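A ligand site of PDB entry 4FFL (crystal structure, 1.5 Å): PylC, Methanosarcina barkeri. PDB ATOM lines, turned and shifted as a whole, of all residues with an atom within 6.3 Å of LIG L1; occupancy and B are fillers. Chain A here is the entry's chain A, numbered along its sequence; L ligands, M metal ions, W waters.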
ATOM      1  N   GLY A   9       8.341  23.198   2.414  1.00  0.00           N
ATOM      2  CA  GLY A   9       9.747  23.568   2.383  1.00  0.00           C
ATOM      3  C   GLY A   9      10.712  22.454   2.025  1.00  0.00           C
ATOM      4  O   GLY A   9      11.800  22.363   2.585  1.00  0.00           O
ATOM      5  N   LYS A  10      10.314  21.602   1.081  1.00  0.00           N
ATOM      6  CA  LYS A  10      11.197  20.556   0.569  1.00  0.00           C
ATOM      7  C   LYS A  10      11.649  20.887  -0.854  1.00  0.00           C
ATOM      8  O   LYS A  10      12.117  21.993  -1.101  1.00  0.00           O
ATOM      9  CB  LYS A  10      10.564  19.165   0.706  1.00  0.00           C
ATOM     10  CG  LYS A  10      10.629  18.608   2.122  1.00  0.00           C
ATOM     11  CD  LYS A  10      10.165  17.168   2.219  1.00  0.00           C
ATOM     12  CE  LYS A  10      11.331  16.194   2.134  1.00  0.00           C
ATOM     13  NZ  LYS A  10      10.933  14.840   2.613  1.00  0.00           N
ATOM     14  N   LEU A  11      11.514  19.942  -1.794  1.00  0.00           N
ATOM     15  CA  LEU A  11      12.104  20.125  -3.122  1.00  0.00           C
ATOM     16  C   LEU A  11      11.361  21.122  -4.007  1.00  0.00           C
ATOM     17  O   LEU A  11      11.989  21.954  -4.661  1.00  0.00           O
ATOM     18  CB  LEU A  11      12.305  18.775  -3.822  1.00  0.00           C
ATOM     19  CG  LEU A  11      13.177  17.769  -3.071  1.00  0.00           C
ATOM     20  CD1 LEU A  11      13.334  16.488  -3.879  1.00  0.00           C
ATOM     21  CD2 LEU A  11      14.535  18.350  -2.708  1.00  0.00           C
ATOM     22  N   GLN A  12      10.030  21.035  -4.033  1.00  0.00           N
ATOM     23  CA  GLN A  12       9.228  22.043  -4.732  1.00  0.00           C
ATOM     24  C   GLN A  12       9.451  23.413  -4.100  1.00  0.00           C
ATOM     25  O   GLN A  12       9.567  24.417  -4.801  1.00  0.00           O
ATOM     26  CB  GLN A  12       7.744  21.720  -4.667  1.00  0.00           C
ATOM     27  CG  GLN A  12       7.296  20.459  -5.385  1.00  0.00           C
ATOM     28  CD  GLN A  12       5.816  20.214  -5.170  1.00  0.00           C
ATOM     29  OE1 GLN A  12       5.430  19.368  -4.363  1.00  0.00           O
ATOM     30  NE2 GLN A  12       4.988  20.990  -5.854  1.00  0.00           N
ATOM     31  N   GLY A  13       9.491  23.421  -2.772  1.00  0.00           N
ATOM     32  CA  GLY A  13       9.707  24.636  -2.001  1.00  0.00           C
ATOM     33  C   GLY A  13      11.026  25.293  -2.356  1.00  0.00           C
ATOM     34  O   GLY A  13      11.075  26.504  -2.559  1.00  0.00           O
ATOM     35  N   VAL A  70       3.346  24.303  -2.254  1.00  0.00           N
ATOM     36  CA  VAL A  70       4.466  23.548  -2.833  1.00  0.00           C
ATOM     37  C   VAL A  70       4.671  22.277  -2.021  1.00  0.00           C
ATOM     38  O   VAL A  70       5.730  22.044  -1.426  1.00  0.00           O
ATOM     39  CB  VAL A  70       5.759  24.382  -2.978  1.00  0.00           C
ATOM     40  CG1 VAL A  70       5.836  25.017  -4.361  1.00  0.00           C
ATOM     41  CG2 VAL A  70       5.863  25.448  -1.886  1.00  0.00           C
ATOM     42  N   ASN A  71       3.624  21.465  -2.001  1.00  0.00           N
ATOM     43  CA  ASN A  71       3.669  20.136  -1.406  1.00  0.00           C
ATOM     44  C   ASN A  71       2.655  19.231  -2.092  1.00  0.00           C
ATOM     45  O   ASN A  71       1.763  19.713  -2.793  1.00  0.00           O
ATOM     46  CB  ASN A  71       3.431  20.199   0.107  1.00  0.00           C
ATOM     47  CG  ASN A  71       1.988  20.526   0.466  1.00  0.00           C
ATOM     48  OD1 ASN A  71       1.123  19.655   0.477  1.00  0.00           O
ATOM     49  ND2 ASN A  71       1.734  21.788   0.803  1.00  0.00           N
ATOM     50  N   GLU A  72       2.812  17.926  -1.894  1.00  0.00           N
ATOM     51  CA  GLU A  72       1.902  16.949  -2.484  1.00  0.00           C
ATOM     52  C   GLU A  72       1.190  16.130  -1.404  1.00  0.00           C
ATOM     53  O   GLU A  72       0.857  14.958  -1.609  1.00  0.00           O
ATOM     54  CB  GLU A  72       2.660  16.047  -3.463  1.00  0.00           C
ATOM     55  CG  GLU A  72       3.226  16.791  -4.660  1.00  0.00           C
ATOM     56  CD  GLU A  72       4.134  15.928  -5.497  1.00  0.00           C
ATOM     57  OE1 GLU A  72       5.213  15.548  -5.014  1.00  0.00           O
ATOM     58  OE2 GLU A  72       3.759  15.631  -6.652  1.00  0.00           O
ATOM     59  N   ASN A  73       0.954  16.760  -0.253  1.00  0.00           N
ATOM     60  CA  ASN A  73       0.152  16.165   0.803  1.00  0.00           C
ATOM     61  C   ASN A  73      -1.314  16.395   0.470  1.00  0.00           C
ATOM     62  O   ASN A  73      -1.804  17.520   0.548  1.00  0.00           O
ATOM     63  CB  ASN A  73       0.523  16.809   2.164  1.00  0.00           C
ATOM     64  CG  ASN A  73      -0.389  16.378   3.302  1.00  0.00           C
ATOM     65  OD1 ASN A  73      -1.223  15.480   3.147  1.00  0.00           O
ATOM     66  ND2 ASN A  73      -0.245  17.018   4.452  1.00  0.00           N
ATOM     67  N   SER A 136       5.336  10.474  -6.622  1.00  0.00           N
ATOM     68  CA  SER A 136       6.180  11.357  -7.419  1.00  0.00           C
ATOM     69  C   SER A 136       7.638  10.950  -7.190  1.00  0.00           C
ATOM     70  O   SER A 136       7.897  10.035  -6.414  1.00  0.00           O
ATOM     71  CB  SER A 136       5.954  12.828  -7.060  1.00  0.00           C
ATOM     72  OG  SER A 136       6.321  13.109  -5.725  1.00  0.00           O
ATOM     73  N   SER A 137       8.565  11.614  -7.887  1.00  0.00           N
ATOM     74  CA  SER A 137      10.011  11.384  -7.716  1.00  0.00           C
ATOM     75  C   SER A 137      10.449   9.954  -8.023  1.00  0.00           C
ATOM     76  O   SER A 137      11.491   9.505  -7.547  1.00  0.00           O
ATOM     77  CB  SER A 137      10.480  11.791  -6.314  1.00  0.00           C
ATOM     78  OG  SER A 137      10.015  13.074  -5.949  1.00  0.00           O
ATOM     79  N   ARG A 243       1.438  21.114 -10.527  1.00  0.00           N
ATOM     80  CA  ARG A 243       1.994  21.750  -9.335  1.00  0.00           C
ATOM     81  C   ARG A 243       3.346  22.302  -9.726  1.00  0.00           C
ATOM     82  O   ARG A 243       3.859  21.988 -10.795  1.00  0.00           O
ATOM     83  CB  ARG A 243       2.094  20.777  -8.141  1.00  0.00           C
ATOM     84  CG  ARG A 243       2.462  19.330  -8.464  1.00  0.00           C
ATOM     85  CD  ARG A 243       3.925  19.114  -8.839  1.00  0.00           C
ATOM     86  NE  ARG A 243       4.335  17.742  -8.551  1.00  0.00           N
ATOM     87  CZ  ARG A 243       5.303  17.077  -9.174  1.00  0.00           C
ATOM     88  NH1 ARG A 243       5.992  17.627 -10.167  1.00  0.00           N
ATOM     89  NH2 ARG A 243       5.579  15.831  -8.795  1.00  0.00           N
ATOM     90  N   PHE A 244       3.920  23.141  -8.864  1.00  0.00           N
ATOM     91  CA  PHE A 244       5.208  23.737  -9.201  1.00  0.00           C
ATOM     92  C   PHE A 244       6.314  22.685  -9.203  1.00  0.00           C
ATOM     93  O   PHE A 244       6.507  22.004  -8.195  1.00  0.00           O
ATOM     94  CB  PHE A 244       5.547  24.917  -8.289  1.00  0.00           C
ATOM     95  CG  PHE A 244       6.559  25.837  -8.886  1.00  0.00           C
ATOM     96  CD1 PHE A 244       6.165  26.903  -9.699  1.00  0.00           C
ATOM     97  CD2 PHE A 244       7.920  25.618  -8.684  1.00  0.00           C
ATOM     98  CE1 PHE A 244       7.098  27.735 -10.281  1.00  0.00           C
ATOM     99  CE2 PHE A 244       8.867  26.453  -9.271  1.00  0.00           C
ATOM    100  CZ  PHE A 244       8.457  27.507 -10.068  1.00  0.00           C
ATOM    101  N   PRO A 245       7.021  22.541 -10.338  1.00  0.00           N
ATOM    102  CA  PRO A 245       8.019  21.477 -10.425  1.00  0.00           C
ATOM    103  C   PRO A 245       9.360  21.831  -9.800  1.00  0.00           C
ATOM    104  O   PRO A 245       9.657  23.010  -9.605  1.00  0.00           O
ATOM    105  CB  PRO A 245       8.165  21.256 -11.928  1.00  0.00           C
ATOM    106  CG  PRO A 245       7.794  22.545 -12.549  1.00  0.00           C
ATOM    107  CD  PRO A 245       6.890  23.293 -11.602  1.00  0.00           C
ATOM    108  N   SER A 246      10.146  20.814  -9.503  1.00  0.00           N
ATOM    109  CA  SER A 246      11.528  20.975  -9.079  1.00  0.00           C
ATOM    110  C   SER A 246      12.460  20.700 -10.266  1.00  0.00           C
ATOM    111  O   SER A 246      12.048  20.084 -11.248  1.00  0.00           O
ATOM    112  CB  SER A 246      11.839  20.008  -7.937  1.00  0.00           C
ATOM    113  OG  SER A 246      11.637  18.672  -8.350  1.00  0.00           O
ATOM    114  N   GLN A 247      13.704  21.188 -10.151  1.00  0.00           N
ATOM    115  CA  GLN A 247      14.787  20.929 -11.113  1.00  0.00           C
ATOM    116  C   GLN A 247      14.654  21.652 -12.458  1.00  0.00           C
ATOM    117  O   GLN A 247      15.498  22.495 -12.804  1.00  0.00           O
ATOM    118  CB  GLN A 247      15.001  19.417 -11.350  1.00  0.00           C
ATOM    119  CG  GLN A 247      15.223  18.607 -10.091  1.00  0.00           C
ATOM    120  CD  GLN A 247      15.381  17.123 -10.361  1.00  0.00           C
ATOM    121  OE1 GLN A 247      16.367  16.509  -9.959  1.00  0.00           O
ATOM    122  NE2 GLN A 247      14.411  16.533 -11.054  1.00  0.00           N
ATOM    123  N   GLU A 302      16.346  12.835  -6.621  1.00  0.00           N
ATOM    124  CA  GLU A 302      15.577  13.585  -5.631  1.00  0.00           C
ATOM    125  C   GLU A 302      15.241  12.817  -4.359  1.00  0.00           C
ATOM    126  O   GLU A 302      15.111  13.422  -3.285  1.00  0.00           O
ATOM    127  CB  GLU A 302      14.294  14.101  -6.259  1.00  0.00           C
ATOM    128  CG  GLU A 302      14.542  15.142  -7.335  1.00  0.00           C
ATOM    129  CD  GLU A 302      13.320  15.984  -7.614  1.00  0.00           C
ATOM    130  OE1 GLU A 302      12.279  15.417  -8.002  1.00  0.00           O
ATOM    131  OE2 GLU A 302      13.404  17.208  -7.427  1.00  0.00           O
ATOM    132  N   SER A 306      15.739  14.380  -0.664  1.00  0.00           N
ATOM    133  CA  SER A 306      14.579  14.427   0.236  1.00  0.00           C
ATOM    134  C   SER A 306      14.881  13.941   1.660  1.00  0.00           C
ATOM    135  O   SER A 306      14.081  14.178   2.577  1.00  0.00           O
ATOM    136  CB  SER A 306      13.420  13.623  -0.363  1.00  0.00           C
ATOM    137  OG  SER A 306      13.662  12.233  -0.288  1.00  0.00           O
HETATM  138  N1  LIG L   1       6.500  17.137  -3.024  1.00  0.00           N
HETATM  139  C1  LIG L   1       7.881  16.638  -2.802  1.00  0.00           C
HETATM  140  C2  LIG L   1       8.798  17.757  -2.362  1.00  0.00           C
HETATM  141  O1  LIG L   1       9.917  17.527  -1.941  1.00  0.00           O
HETATM  142  C3  LIG L   1       8.389  15.920  -4.082  1.00  0.00           C
HETATM  143  C4  LIG L   1       8.517  16.852  -5.316  1.00  0.00           C
HETATM  144  C5  LIG L   1       9.149  16.087  -6.512  1.00  0.00           C
HETATM  145  C6  LIG L   1       9.003  16.886  -7.831  1.00  0.00           C
HETATM  146  N2  LIG L   1       9.933  16.358  -8.850  1.00  0.00           N
HETATM  147  O2  LIG L   1       8.316  18.997  -2.503  1.00  0.00           O
HETATM  148  P1  LG2 L   2       7.510  14.395   4.243  1.00  0.00           P
HETATM  149  O1  LG2 L   2       7.590  12.937   3.869  1.00  0.00           O
HETATM  150  O2  LG2 L   2       8.785  14.971   4.800  1.00  0.00           O
HETATM  151  O3  LG2 L   2       6.271  14.761   5.042  1.00  0.00           O
HETATM  152  P2  LG2 L   2       7.356  14.525   1.379  1.00  0.00           P
HETATM  153  O4  LG2 L   2       8.791  14.293   0.978  1.00  0.00           O
HETATM  154  O5  LG2 L   2       6.386  13.386   1.268  1.00  0.00           O
HETATM  155  O6  LG2 L   2       7.305  15.192   2.854  1.00  0.00           O
HETATM  156  P3  LG2 L   2       5.409  16.507   0.638  1.00  0.00           P
HETATM  157  O7  LG2 L   2       4.373  15.624   1.290  1.00  0.00           O
HETATM  158  O8  LG2 L   2       5.105  17.119  -0.710  1.00  0.00           O
HETATM  159  O9  LG2 L   2       6.831  15.769   0.498  1.00  0.00           O
HETATM  160  O10 LG2 L   2       5.697  17.717   1.658  1.00  0.00           O
HETATM  161  C1  LG2 L   2       6.606  18.757   1.322  1.00  0.00           C
HETATM  162  C2  LG2 L   2       6.714  19.695   2.512  1.00  0.00           C
HETATM  163  O11 LG2 L   2       5.427  20.262   2.792  1.00  0.00           O
HETATM  164  C3  LG2 L   2       7.182  18.955   3.761  1.00  0.00           C
HETATM  165  O12 LG2 L   2       8.312  19.624   4.325  1.00  0.00           O
HETATM  166  C4  LG2 L   2       5.969  19.002   4.689  1.00  0.00           C
HETATM  167  O13 LG2 L   2       6.325  19.063   6.070  1.00  0.00           O
HETATM  168  C5  LG2 L   2       5.210  20.231   4.192  1.00  0.00           C
HETATM  169  N1  LG2 L   2       3.772  20.088   4.510  1.00  0.00           N
HETATM  170  C6  LG2 L   2       2.948  19.095   4.109  1.00  0.00           C
HETATM  171  N2  LG2 L   2       1.707  19.264   4.613  1.00  0.00           N
HETATM  172  C7  LG2 L   2       1.725  20.384   5.353  1.00  0.00           C
HETATM  173  C8  LG2 L   2       0.740  21.141   6.172  1.00  0.00           C
HETATM  174  N3  LG2 L   2      -0.531  20.705   6.283  1.00  0.00           N
HETATM  175  N4  LG2 L   2       1.172  22.274   6.781  1.00  0.00           N
HETATM  176  C9  LG2 L   2       2.446  22.701   6.673  1.00  0.00           C
HETATM  177  N5  LG2 L   2       3.390  22.072   5.954  1.00  0.00           N
HETATM  178  C10 LG2 L   2       3.091  20.928   5.294  1.00  0.00           C
HETATM  179  P1  LG3 L   3       6.603  10.490 -11.365  1.00  0.00           P
HETATM  180  O1  LG3 L   3       5.352  10.686 -10.580  1.00  0.00           O
HETATM  181  O2  LG3 L   3       7.084   9.449 -10.377  1.00  0.00           O
HETATM  182  O3  LG3 L   3       7.922  11.154 -11.397  1.00  0.00           O
HETATM  183  P2  LG3 L   3       6.558   8.980 -13.911  1.00  0.00           P
HETATM  184  O4  LG3 L   3       5.327   8.388 -14.558  1.00  0.00           O
HETATM  185  O5  LG3 L   3       7.136  10.179 -14.582  1.00  0.00           O
HETATM  186  O6  LG3 L   3       6.213   9.271 -12.375  1.00  0.00           O
HETATM  187  O7  LG3 L   3       7.680   7.836 -13.866  1.00  0.00           O
HETATM  188  C1  LG3 L   3       8.954   8.097 -13.266  1.00  0.00           C
HETATM  189  C2  LG3 L   3      10.072   7.704 -14.203  1.00  0.00           C
HETATM  190  O8  LG3 L   3       9.947   6.321 -14.559  1.00  0.00           O
HETATM  191  C3  LG3 L   3      10.051   8.458 -15.531  1.00  0.00           C
HETATM  192  O9  LG3 L   3      10.757   9.696 -15.494  1.00  0.00           O
HETATM  193  C4  LG3 L   3      10.677   7.473 -16.492  1.00  0.00           C
HETATM  194  O10 LG3 L   3      12.098   7.543 -16.391  1.00  0.00           O
HETATM  195  C5  LG3 L   3      10.236   6.130 -15.946  1.00  0.00           C
HETATM  196  N1  LG3 L   3       9.016   5.605 -16.600  1.00  0.00           N
HETATM  197  C6  LG3 L   3       7.734   5.834 -16.249  1.00  0.00           C
HETATM  198  N2  LG3 L   3       6.875   5.162 -17.049  1.00  0.00           N
HETATM  199  C7  LG3 L   3       7.618   4.480 -17.940  1.00  0.00           C
HETATM  200  C8  LG3 L   3       7.340   3.563 -19.067  1.00  0.00           C
HETATM  201  N3  LG3 L   3       6.080   3.234 -19.415  1.00  0.00           N
HETATM  202  N4  LG3 L   3       8.413   3.052 -19.738  1.00  0.00           N
HETATM  203  C9  LG3 L   3       9.682   3.359 -19.408  1.00  0.00           C
HETATM  204  N5  LG3 L   3      10.001   4.189 -18.394  1.00  0.00           N
HETATM  205  C10 LG3 L   3       9.023   4.762 -17.634  1.00  0.00           C
HETATM  206 MG    MG M   1       8.350  15.620 -12.814  1.00  0.00          MG
HETATM  207  O   HOH W   1      10.534  14.985  -1.212  1.00  0.00           O
HETATM  208  O   HOH W   2       6.481  13.701  -2.058  1.00  0.00           O
HETATM  209  O   HOH W   3       8.344  21.261  -1.051  1.00  0.00           O
HETATM  210  O   HOH W   4       9.609  18.355 -10.770  1.00  0.00           O
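Merely in contact with LIG L1: Lys 10, Ser 136, Ser 137 and Arg 243. Hydrophobic or aromatic side chains within 4 Å of LIG L1: Leu 11. Nine residues have an atom within 4 Å of LIG L1: Lys 10, Leu 11, Gln 12, Glu 72, Ser 136, Ser 137, Arg 243, Ser 246 and Glu 302. Along chain A the residues within 4 Å of LIG L1 span positions 10 to 302. The nearest printed residue that does not touch LIG L1 is Val 70 (4.1 Å).
A nitrogen (N1) of LIG L1 is in hydrogen-bond range of an oxygen (O8) of LG2 L2, at 2.7 Å.
OE2 of Glu 302 sits at hydrogen-bond distance from OG of Ser 246, 2.5 Å away. NE2 of Gln 12 lies within hydrogen-bond range of O of Phe 244, at 3.0 Å. OE2 of Glu 72 lies within salt-bridge range of NH2 of Arg 243 (2.8 Å). The side-chain carboxylate (OE1) of Glu 72 lies within hydrogen-bond range of the side-chain hydroxyl (OG) of Ser 136 (2.8 Å). The side-chain amino group (NZ) of Lys 10 lies within hydrogen-bond range of the backbone carbonyl oxygen (O) of Ser 306, at 3.2 Å.
OE1 of Glu 302 lies within salt-bridge range of N2 of LIG L1. The backbone NH (N) of Gln 12 is in hydrogen-bond range of an oxygen (O2) of LIG L1 (3.1 Å). The side-chain amide oxygen (OE1) of Gln 12 is in hydrogen-bond range of a nitrogen (N1) of LIG L1 (2.8 Å). The side-chain carboxylate (OE1) of Glu 72 is in salt-bridge range of a nitrogen (N1) of LIG L1. An oxygen (O1) of LIG L1 sits at hydrogen-bond distance from the backbone NH (N) of Leu 11 (2.9 Å). N2 of LIG L1 lies within hydrogen-bond range of OG of Ser 246 (2.9 Å). N of Glu 72 lies within hydrogen-bond range of O8 of LG2 L2. An oxygen (O4) of LG2 L2 is in salt-bridge range of the side-chain amino group (NZ) of Lys 10 (2.7 Å). N2 of LG2 L2 is in hydrogen-bond range of ND2 of Asn 73, at 3.0 Å.
Water W1 bridges O1 of LIG L1 and O4 of LG2 L2. Water W4 lies within hydrogen-bond range of N2 of LIG L1 (2.8 Å) and N of Ser 246 (2.8 Å).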
